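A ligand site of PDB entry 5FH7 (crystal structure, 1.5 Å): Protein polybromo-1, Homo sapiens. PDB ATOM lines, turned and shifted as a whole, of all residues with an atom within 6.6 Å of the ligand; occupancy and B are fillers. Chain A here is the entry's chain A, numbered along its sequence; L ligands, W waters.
The side-chain hydroxyl of Tyr 54 lies within hydrogen-bond range of an oxygen (O1) of the ligand (2.7 Å).
The side-chain amide nitrogen of Asn 97 lies close to a nitrogen (N2) of the ligand (3.2 Å).
Water W1 lies within hydrogen-bond range of the side-chain hydroxyl of Tyr 54 (2.8 Å), the backbone carbonyl oxygen of Met 62 (2.8 Å) and the side-chain amide nitrogen of Asn 92 (2.9 Å).
The side-chain carboxylate of Asp 63 is in hydrogen-bond range of the backbone NH of Leu 45, 2.8 Å away.
O of Phe 42 sits at hydrogen-bond distance from N of Met 64 (3.0 Å).
The backbone carbonyl oxygen of Ala 93 is in hydrogen-bond range of the side-chain amide nitrogen of Asn 97.
Ile 41 touches the ligand (O to C5, 3.1 Å).
CA of Phe 42 touches C6 of the ligand, 3.6 Å away.
CD1 of Leu 45 touches C3 of the ligand, at 3.6 Å.
CD of Pro 46 touches C2 of the ligand (3.6 Å).
Leu 51 touches the ligand (CD2 to N3, 3.8 Å).
O of Met 62 touches C7 of the ligand (3.5 Å).
O of Met 89 touches CL1 of the ligand (3.2 Å).
CA of Ala 93 touches O1 of the ligand, 3.2 Å away.
CE2 of Tyr 96 touches C14 of the ligand, 3.9 Å away.
Ile 103 touches the ligand.
Hydrophobic or aromatic side chains that line the ligand: Ile 41, Phe 42, Leu 45, Pro 46, Leu 51, Tyr 54, Met 89, Ala 93, Tyr 96 and Ile 103.
Within 4 Å of the ligand: Ile 41, Phe 42, Leu 45, Pro 46, Leu 51, Tyr 54, Met 62, Met 89, Ala 93, Tyr 96, Asn 97 and Ile 103.
The nearest printed residue that does not touch the ligand is Asn 92 (4.1 Å).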
ATOM      1  N   ILE A  41     -17.830 -29.840 -17.382  1.00  0.00           N
ATOM      2  CA  ILE A  41     -17.799 -28.514 -16.792  1.00  0.00           C
ATOM      3  C   ILE A  41     -19.195 -28.106 -16.304  1.00  0.00           C
ATOM      4  O   ILE A  41     -19.310 -27.243 -15.431  1.00  0.00           O
ATOM      5  CB  ILE A  41     -17.224 -27.463 -17.801  1.00  0.00           C
ATOM      6  CG1 ILE A  41     -16.871 -26.117 -17.154  1.00  0.00           C
ATOM      7  CG2 ILE A  41     -18.149 -27.150 -18.953  1.00  0.00           C
ATOM      8  CD1 ILE A  41     -15.695 -26.207 -16.210  1.00  0.00           C
ATOM      9  N   PHE A  42     -20.261 -28.642 -16.890  1.00  0.00           N
ATOM     10  CA  PHE A  42     -21.619 -28.213 -16.614  1.00  0.00           C
ATOM     11  C   PHE A  42     -22.279 -28.874 -15.420  1.00  0.00           C
ATOM     12  O   PHE A  42     -23.372 -28.527 -15.054  1.00  0.00           O
ATOM     13  CB  PHE A  42     -22.509 -28.442 -17.845  1.00  0.00           C
ATOM     14  CG  PHE A  42     -22.088 -27.663 -19.079  1.00  0.00           C
ATOM     15  CD1 PHE A  42     -22.320 -26.317 -19.163  1.00  0.00           C
ATOM     16  CD2 PHE A  42     -21.366 -28.240 -20.087  1.00  0.00           C
ATOM     17  CE1 PHE A  42     -21.959 -25.611 -20.316  1.00  0.00           C
ATOM     18  CE2 PHE A  42     -20.941 -27.529 -21.204  1.00  0.00           C
ATOM     19  CZ  PHE A  42     -21.234 -26.170 -21.297  1.00  0.00           C
ATOM     20  N   LEU A  43     -21.603 -29.860 -14.800  1.00  0.00           N
ATOM     21  CA  LEU A  43     -22.256 -30.584 -13.731  1.00  0.00           C
ATOM     22  C   LEU A  43     -22.595 -29.744 -12.520  1.00  0.00           C
ATOM     23  O   LEU A  43     -23.701 -29.769 -12.046  1.00  0.00           O
ATOM     24  CB  LEU A  43     -21.445 -31.824 -13.333  1.00  0.00           C
ATOM     25  CG  LEU A  43     -21.100 -32.840 -14.439  1.00  0.00           C
ATOM     26  CD1 LEU A  43     -20.505 -34.053 -13.745  1.00  0.00           C
ATOM     27  CD2 LEU A  43     -22.282 -33.332 -15.205  1.00  0.00           C
ATOM     28  N   ARG A  44     -21.653 -28.917 -12.097  1.00  0.00           N
ATOM     29  CA  ARG A  44     -21.860 -28.065 -10.950  1.00  0.00           C
ATOM     30  C   ARG A  44     -21.248 -26.685 -11.155  1.00  0.00           C
ATOM     31  O   ARG A  44     -20.042 -26.528 -11.385  1.00  0.00           O
ATOM     32  CB  ARG A  44     -21.235 -28.718  -9.683  1.00  0.00           C
ATOM     33  CG  ARG A  44     -21.567 -27.986  -8.441  1.00  0.00           C
ATOM     34  CD  ARG A  44     -23.003 -28.259  -7.999  1.00  0.00           C
ATOM     35  NE  ARG A  44     -23.244 -27.557  -6.721  1.00  0.00           N
ATOM     36  CZ  ARG A  44     -23.784 -26.353  -6.569  1.00  0.00           C
ATOM     37  NH1 ARG A  44     -24.293 -25.623  -7.596  1.00  0.00           N
ATOM     38  NH2 ARG A  44     -23.868 -25.841  -5.342  1.00  0.00           N
ATOM     39  N   LEU A  45     -22.080 -25.647 -10.975  1.00  0.00           N
ATOM     40  CA  LEU A  45     -21.604 -24.271 -11.095  1.00  0.00           C
ATOM     41  C   LEU A  45     -20.720 -23.951  -9.911  1.00  0.00           C
ATOM     42  O   LEU A  45     -21.105 -24.329  -8.806  1.00  0.00           O
ATOM     43  CB  LEU A  45     -22.810 -23.341 -11.119  1.00  0.00           C
ATOM     44  CG  LEU A  45     -22.590 -21.915 -11.649  1.00  0.00           C
ATOM     45  CD1 LEU A  45     -22.042 -21.787 -13.036  1.00  0.00           C
ATOM     46  CD2 LEU A  45     -23.840 -21.046 -11.526  1.00  0.00           C
ATOM     47  N   PRO A  46     -19.555 -23.292 -10.125  1.00  0.00           N
ATOM     48  CA  PRO A  46     -18.752 -22.769  -9.035  1.00  0.00           C
ATOM     49  C   PRO A  46     -19.466 -21.654  -8.271  1.00  0.00           C
ATOM     50  O   PRO A  46     -20.559 -21.259  -8.646  1.00  0.00           O
ATOM     51  CB  PRO A  46     -17.531 -22.237  -9.771  1.00  0.00           C
ATOM     52  CG  PRO A  46     -17.457 -22.979 -11.055  1.00  0.00           C
ATOM     53  CD  PRO A  46     -18.885 -23.170 -11.425  1.00  0.00           C
ATOM     54  N   GLU A  50     -15.379 -17.840  -7.215  1.00  0.00           N
ATOM     55  CA  GLU A  50     -14.701 -18.482  -8.315  1.00  0.00           C
ATOM     56  C   GLU A  50     -14.995 -17.888  -9.659  1.00  0.00           C
ATOM     57  O   GLU A  50     -14.138 -17.950 -10.569  1.00  0.00           O
ATOM     58  CB  GLU A  50     -15.030 -20.017  -8.272  1.00  0.00           C
ATOM     59  CG  GLU A  50     -14.588 -20.711  -6.964  1.00  0.00           C
ATOM     60  CD  GLU A  50     -15.109 -22.138  -6.740  1.00  0.00           C
ATOM     61  OE1 GLU A  50     -16.323 -22.391  -6.803  1.00  0.00           O
ATOM     62  OE2 GLU A  50     -14.288 -23.059  -6.438  1.00  0.00           O
ATOM     63  N   LEU A  51     -16.202 -17.342  -9.859  1.00  0.00           N
ATOM     64  CA  LEU A  51     -16.555 -16.747 -11.137  1.00  0.00           C
ATOM     65  C   LEU A  51     -17.122 -15.381 -10.791  1.00  0.00           C
ATOM     66  O   LEU A  51     -18.333 -15.249 -10.669  1.00  0.00           O
ATOM     67  CB  LEU A  51     -17.588 -17.577 -11.893  1.00  0.00           C
ATOM     68  CG  LEU A  51     -17.155 -18.975 -12.286  1.00  0.00           C
ATOM     69  CD1 LEU A  51     -18.350 -19.740 -12.807  1.00  0.00           C
ATOM     70  CD2 LEU A  51     -16.062 -18.928 -13.346  1.00  0.00           C
ATOM     71  N   TYR A  54     -20.081 -13.912 -12.424  1.00  0.00           N
ATOM     72  CA  TYR A  54     -21.125 -14.849 -12.947  1.00  0.00           C
ATOM     73  C   TYR A  54     -22.511 -14.599 -12.400  1.00  0.00           C
ATOM     74  O   TYR A  54     -23.477 -14.443 -13.113  1.00  0.00           O
ATOM     75  CB  TYR A  54     -20.770 -16.317 -12.670  1.00  0.00           C
ATOM     76  CG  TYR A  54     -21.518 -17.283 -13.560  1.00  0.00           C
ATOM     77  CD1 TYR A  54     -22.776 -17.730 -13.240  1.00  0.00           C
ATOM     78  CD2 TYR A  54     -20.942 -17.744 -14.745  1.00  0.00           C
ATOM     79  CE1 TYR A  54     -23.466 -18.610 -14.098  1.00  0.00           C
ATOM     80  CE2 TYR A  54     -21.630 -18.600 -15.597  1.00  0.00           C
ATOM     81  CZ  TYR A  54     -22.886 -19.000 -15.266  1.00  0.00           C
ATOM     82  OH  TYR A  54     -23.551 -19.854 -16.114  1.00  0.00           O
ATOM     83  N   ILE A  58     -25.676 -13.337 -14.613  1.00  0.00           N
ATOM     84  CA  ILE A  58     -26.571 -14.441 -15.013  1.00  0.00           C
ATOM     85  C   ILE A  58     -27.752 -14.456 -14.054  1.00  0.00           C
ATOM     86  O   ILE A  58     -27.579 -14.857 -12.897  1.00  0.00           O
ATOM     87  CB  ILE A  58     -25.832 -15.799 -15.035  1.00  0.00           C
ATOM     88  CG1 ILE A  58     -24.675 -15.746 -16.059  1.00  0.00           C
ATOM     89  CG2 ILE A  58     -26.799 -16.952 -15.367  1.00  0.00           C
ATOM     90  CD1 ILE A  58     -25.050 -15.359 -17.490  1.00  0.00           C
ATOM     91  N   MET A  62     -27.903 -22.132 -13.508  1.00  0.00           N
ATOM     92  CA  MET A  62     -28.398 -23.488 -13.764  1.00  0.00           C
ATOM     93  C   MET A  62     -27.216 -24.395 -14.000  1.00  0.00           C
ATOM     94  O   MET A  62     -26.234 -24.031 -14.636  1.00  0.00           O
ATOM     95  CB  MET A  62     -29.285 -23.477 -15.023  1.00  0.00           C
ATOM     96  CG  MET A  62     -29.990 -24.793 -15.311  1.00  0.00           C
ATOM     97  SD  MET A  62     -31.037 -25.449 -14.006  1.00  0.00           S
ATOM     98  CE  MET A  62     -32.143 -24.081 -13.900  1.00  0.00           C
ATOM     99  N   ASP A  63     -27.275 -25.621 -13.433  1.00  0.00           N
ATOM    100  CA  ASP A  63     -26.316 -26.640 -13.740  1.00  0.00           C
ATOM    101  C   ASP A  63     -26.974 -27.968 -13.807  1.00  0.00           C
ATOM    102  O   ASP A  63     -28.142 -28.090 -13.519  1.00  0.00           O
ATOM    103  CB  ASP A  63     -25.133 -26.566 -12.767  1.00  0.00           C
ATOM    104  CG  ASP A  63     -25.487 -26.796 -11.311  1.00  0.00           C
ATOM    105  OD1 ASP A  63     -26.488 -27.468 -11.007  1.00  0.00           O
ATOM    106  OD2 ASP A  63     -24.694 -26.312 -10.400  1.00  0.00           O
ATOM    107  N   MET A  64     -26.222 -28.987 -14.233  1.00  0.00           N
ATOM    108  CA  MET A  64     -26.807 -30.316 -14.421  1.00  0.00           C
ATOM    109  C   MET A  64     -27.159 -30.978 -13.111  1.00  0.00           C
ATOM    110  O   MET A  64     -28.110 -31.694 -13.103  1.00  0.00           O
ATOM    111  CB  MET A  64     -25.917 -31.180 -15.297  1.00  0.00           C
ATOM    112  CG  MET A  64     -25.935 -30.644 -16.715  1.00  0.00           C
ATOM    113  SD  MET A  64     -25.070 -31.675 -17.919  1.00  0.00           S
ATOM    114  CE  MET A  64     -25.995 -33.204 -17.810  1.00  0.00           C
ATOM    115  N   MET A  88     -31.767 -23.032 -20.791  1.00  0.00           N
ATOM    116  CA  MET A  88     -31.342 -21.966 -19.908  1.00  0.00           C
ATOM    117  C   MET A  88     -29.866 -22.069 -19.606  1.00  0.00           C
ATOM    118  O   MET A  88     -29.089 -21.115 -19.693  1.00  0.00           O
ATOM    119  CB  MET A  88     -32.194 -21.958 -18.601  1.00  0.00           C
ATOM    120  CG  MET A  88     -31.733 -20.875 -17.604  1.00  0.00           C
ATOM    121  SD  MET A  88     -32.004 -19.169 -18.136  1.00  0.00           S
ATOM    122  CE  MET A  88     -33.768 -19.147 -18.197  1.00  0.00           C
ATOM    123  N   MET A  89     -29.426 -23.276 -19.243  1.00  0.00           N
ATOM    124  CA  MET A  89     -28.024 -23.509 -18.919  1.00  0.00           C
ATOM    125  C   MET A  89     -27.130 -23.148 -20.109  1.00  0.00           C
ATOM    126  O   MET A  89     -26.112 -22.525 -19.947  1.00  0.00           O
ATOM    127  CB  MET A  89     -27.863 -24.985 -18.469  1.00  0.00           C
ATOM    128  CG  MET A  89     -26.489 -25.294 -17.989  1.00  0.00           C
ATOM    129  SD  MET A  89     -26.283 -27.007 -17.503  1.00  0.00           S
ATOM    130  CE  MET A  89     -26.109 -27.727 -19.128  1.00  0.00           C
ATOM    131  N   PHE A  90     -27.514 -23.588 -21.313  1.00  0.00           N
ATOM    132  CA  PHE A  90     -26.690 -23.298 -22.504  1.00  0.00           C
ATOM    133  C   PHE A  90     -26.689 -21.837 -22.874  1.00  0.00           C
ATOM    134  O   PHE A  90     -25.663 -21.311 -23.207  1.00  0.00           O
ATOM    135  CB  PHE A  90     -27.101 -24.254 -23.685  1.00  0.00           C
ATOM    136  CG  PHE A  90     -26.978 -25.721 -23.374  1.00  0.00           C
ATOM    137  CD1 PHE A  90     -25.834 -26.221 -22.739  1.00  0.00           C
ATOM    138  CD2 PHE A  90     -28.000 -26.588 -23.749  1.00  0.00           C
ATOM    139  CE1 PHE A  90     -25.711 -27.627 -22.493  1.00  0.00           C
ATOM    140  CE2 PHE A  90     -27.868 -27.948 -23.524  1.00  0.00           C
ATOM    141  CZ  PHE A  90     -26.756 -28.438 -22.904  1.00  0.00           C
ATOM    142  N   ASN A  91     -27.825 -21.169 -22.749  1.00  0.00           N
ATOM    143  CA  ASN A  91     -27.861 -19.734 -22.959  1.00  0.00           C
ATOM    144  C   ASN A  91     -26.997 -19.051 -21.926  1.00  0.00           C
ATOM    145  O   ASN A  91     -26.336 -18.061 -22.254  1.00  0.00           O
ATOM    146  CB  ASN A  91     -29.299 -19.178 -22.909  1.00  0.00           C
ATOM    147  CG  ASN A  91     -30.052 -19.312 -24.222  1.00  0.00           C
ATOM    148  OD1 ASN A  91     -31.271 -19.711 -24.287  1.00  0.00           O
ATOM    149  ND2 ASN A  91     -29.395 -19.004 -25.304  1.00  0.00           N
ATOM    150  N   ASN A  92     -27.018 -19.484 -20.675  1.00  0.00           N
ATOM    151  CA  ASN A  92     -26.183 -18.874 -19.663  1.00  0.00           C
ATOM    152  C   ASN A  92     -24.719 -19.022 -20.019  1.00  0.00           C
ATOM    153  O   ASN A  92     -23.938 -18.091 -19.913  1.00  0.00           O
ATOM    154  CB  ASN A  92     -26.425 -19.552 -18.313  1.00  0.00           C
ATOM    155  CG  ASN A  92     -27.773 -19.253 -17.658  1.00  0.00           C
ATOM    156  OD1 ASN A  92     -28.534 -18.355 -18.095  1.00  0.00           O
ATOM    157  ND2 ASN A  92     -28.063 -19.967 -16.613  1.00  0.00           N
ATOM    158  N   ALA A  93     -24.334 -20.247 -20.402  1.00  0.00           N
ATOM    159  CA  ALA A  93     -22.934 -20.513 -20.793  1.00  0.00           C
ATOM    160  C   ALA A  93     -22.496 -19.629 -21.958  1.00  0.00           C
ATOM    161  O   ALA A  93     -21.402 -19.062 -21.939  1.00  0.00           O
ATOM    162  CB  ALA A  93     -22.721 -21.976 -21.163  1.00  0.00           C
ATOM    163  N   CYS A  94     -23.396 -19.408 -22.920  1.00  0.00           N
ATOM    164  CA  CYS A  94     -23.034 -18.605 -24.092  1.00  0.00           C
ATOM    165  C   CYS A  94     -23.144 -17.110 -23.836  1.00  0.00           C
ATOM    166  O   CYS A  94     -22.647 -16.293 -24.646  1.00  0.00           O
ATOM    167  CB  CYS A  94     -23.855 -19.024 -25.281  1.00  0.00           C
ATOM    168  SG  CYS A  94     -23.530 -20.702 -25.855  1.00  0.00           S
ATOM    169  N   TYR A  96     -22.106 -15.825 -20.588  1.00  0.00           N
ATOM    170  CA  TYR A  96     -20.930 -15.547 -19.747  1.00  0.00           C
ATOM    171  C   TYR A  96     -19.623 -15.743 -20.423  1.00  0.00           C
ATOM    172  O   TYR A  96     -18.671 -14.944 -20.227  1.00  0.00           O
ATOM    173  CB  TYR A  96     -20.956 -16.484 -18.512  1.00  0.00           C
ATOM    174  CG  TYR A  96     -19.900 -16.122 -17.534  1.00  0.00           C
ATOM    175  CD1 TYR A  96     -20.039 -14.994 -16.729  1.00  0.00           C
ATOM    176  CD2 TYR A  96     -18.783 -16.899 -17.403  1.00  0.00           C
ATOM    177  CE1 TYR A  96     -19.039 -14.678 -15.833  1.00  0.00           C
ATOM    178  CE2 TYR A  96     -17.780 -16.585 -16.476  1.00  0.00           C
ATOM    179  CZ  TYR A  96     -17.933 -15.498 -15.712  1.00  0.00           C
ATOM    180  OH  TYR A  96     -16.897 -15.203 -14.800  1.00  0.00           O
ATOM    181  N   ASN A  97     -19.534 -16.784 -21.243  1.00  0.00           N
ATOM    182  CA  ASN A  97     -18.306 -17.150 -21.961  1.00  0.00           C
ATOM    183  C   ASN A  97     -18.266 -16.591 -23.367  1.00  0.00           C
ATOM    184  O   ASN A  97     -19.310 -16.336 -23.945  1.00  0.00           O
ATOM    185  CB  ASN A  97     -18.179 -18.646 -21.928  1.00  0.00           C
ATOM    186  CG  ASN A  97     -18.162 -19.189 -20.498  1.00  0.00           C
ATOM    187  OD1 ASN A  97     -17.105 -19.126 -19.828  1.00  0.00           O
ATOM    188  ND2 ASN A  97     -19.282 -19.719 -20.017  1.00  0.00           N
ATOM    189  N   ILE A 103     -15.909 -23.694 -23.595  1.00  0.00           N
ATOM    190  CA  ILE A 103     -17.205 -23.917 -22.965  1.00  0.00           C
ATOM    191  C   ILE A 103     -18.359 -23.474 -23.879  1.00  0.00           C
ATOM    192  O   ILE A 103     -19.397 -24.157 -23.972  1.00  0.00           O
ATOM    193  CB  ILE A 103     -17.304 -23.245 -21.609  1.00  0.00           C
ATOM    194  CG1 ILE A 103     -18.660 -23.526 -20.965  1.00  0.00           C
ATOM    195  CG2 ILE A 103     -17.167 -21.816 -21.691  1.00  0.00           C
ATOM    196  CD1 ILE A 103     -18.567 -23.480 -19.469  1.00  0.00           C
HETATM  197  C1  LIG L   1     -16.796 -22.736 -15.398  1.00  0.00           C
HETATM  198  C2  LIG L   1     -18.007 -23.497 -14.913  1.00  0.00           C
HETATM  199  C3  LIG L   1     -20.405 -23.453 -15.739  1.00  0.00           C
HETATM  200  C4  LIG L   1     -21.327 -22.770 -16.567  1.00  0.00           C
HETATM  201  C5  LIG L   1     -20.778 -24.553 -14.966  1.00  0.00           C
HETATM  202  C6  LIG L   1     -22.071 -25.015 -15.011  1.00  0.00           C
HETATM  203  C7  LIG L   1     -22.992 -24.405 -15.814  1.00  0.00           C
HETATM  204  C8  LIG L   1     -22.619 -23.322 -16.605  1.00  0.00           C
HETATM  205  C9  LIG L   1     -20.879 -21.554 -17.297  1.00  0.00           C
HETATM  206  C10 LIG L   1     -18.704 -21.869 -16.459  1.00  0.00           C
HETATM  207  N1  LIG L   1     -19.109 -22.955 -15.722  1.00  0.00           N
HETATM  208  N2  LIG L   1     -19.533 -21.198 -17.222  1.00  0.00           N
HETATM  209  C11 LIG L   1     -17.321 -21.631 -16.265  1.00  0.00           C
HETATM  210 CL1  LIG L   1     -23.835 -22.748 -17.708  1.00  0.00          CL
HETATM  211  O1  LIG L   1     -21.685 -20.778 -17.866  1.00  0.00           O
HETATM  212  C12 LIG L   1     -16.672 -20.584 -16.800  1.00  0.00           C
HETATM  213  N3  LIG L   1     -15.393 -20.225 -16.814  1.00  0.00           N
HETATM  214  C13 LIG L   1     -14.286 -21.049 -16.253  1.00  0.00           C
HETATM  215  C14 LIG L   1     -14.931 -19.007 -17.443  1.00  0.00           C
HETATM  216  O   HOH W   1     -25.777 -21.331 -15.345  1.00  0.00           O
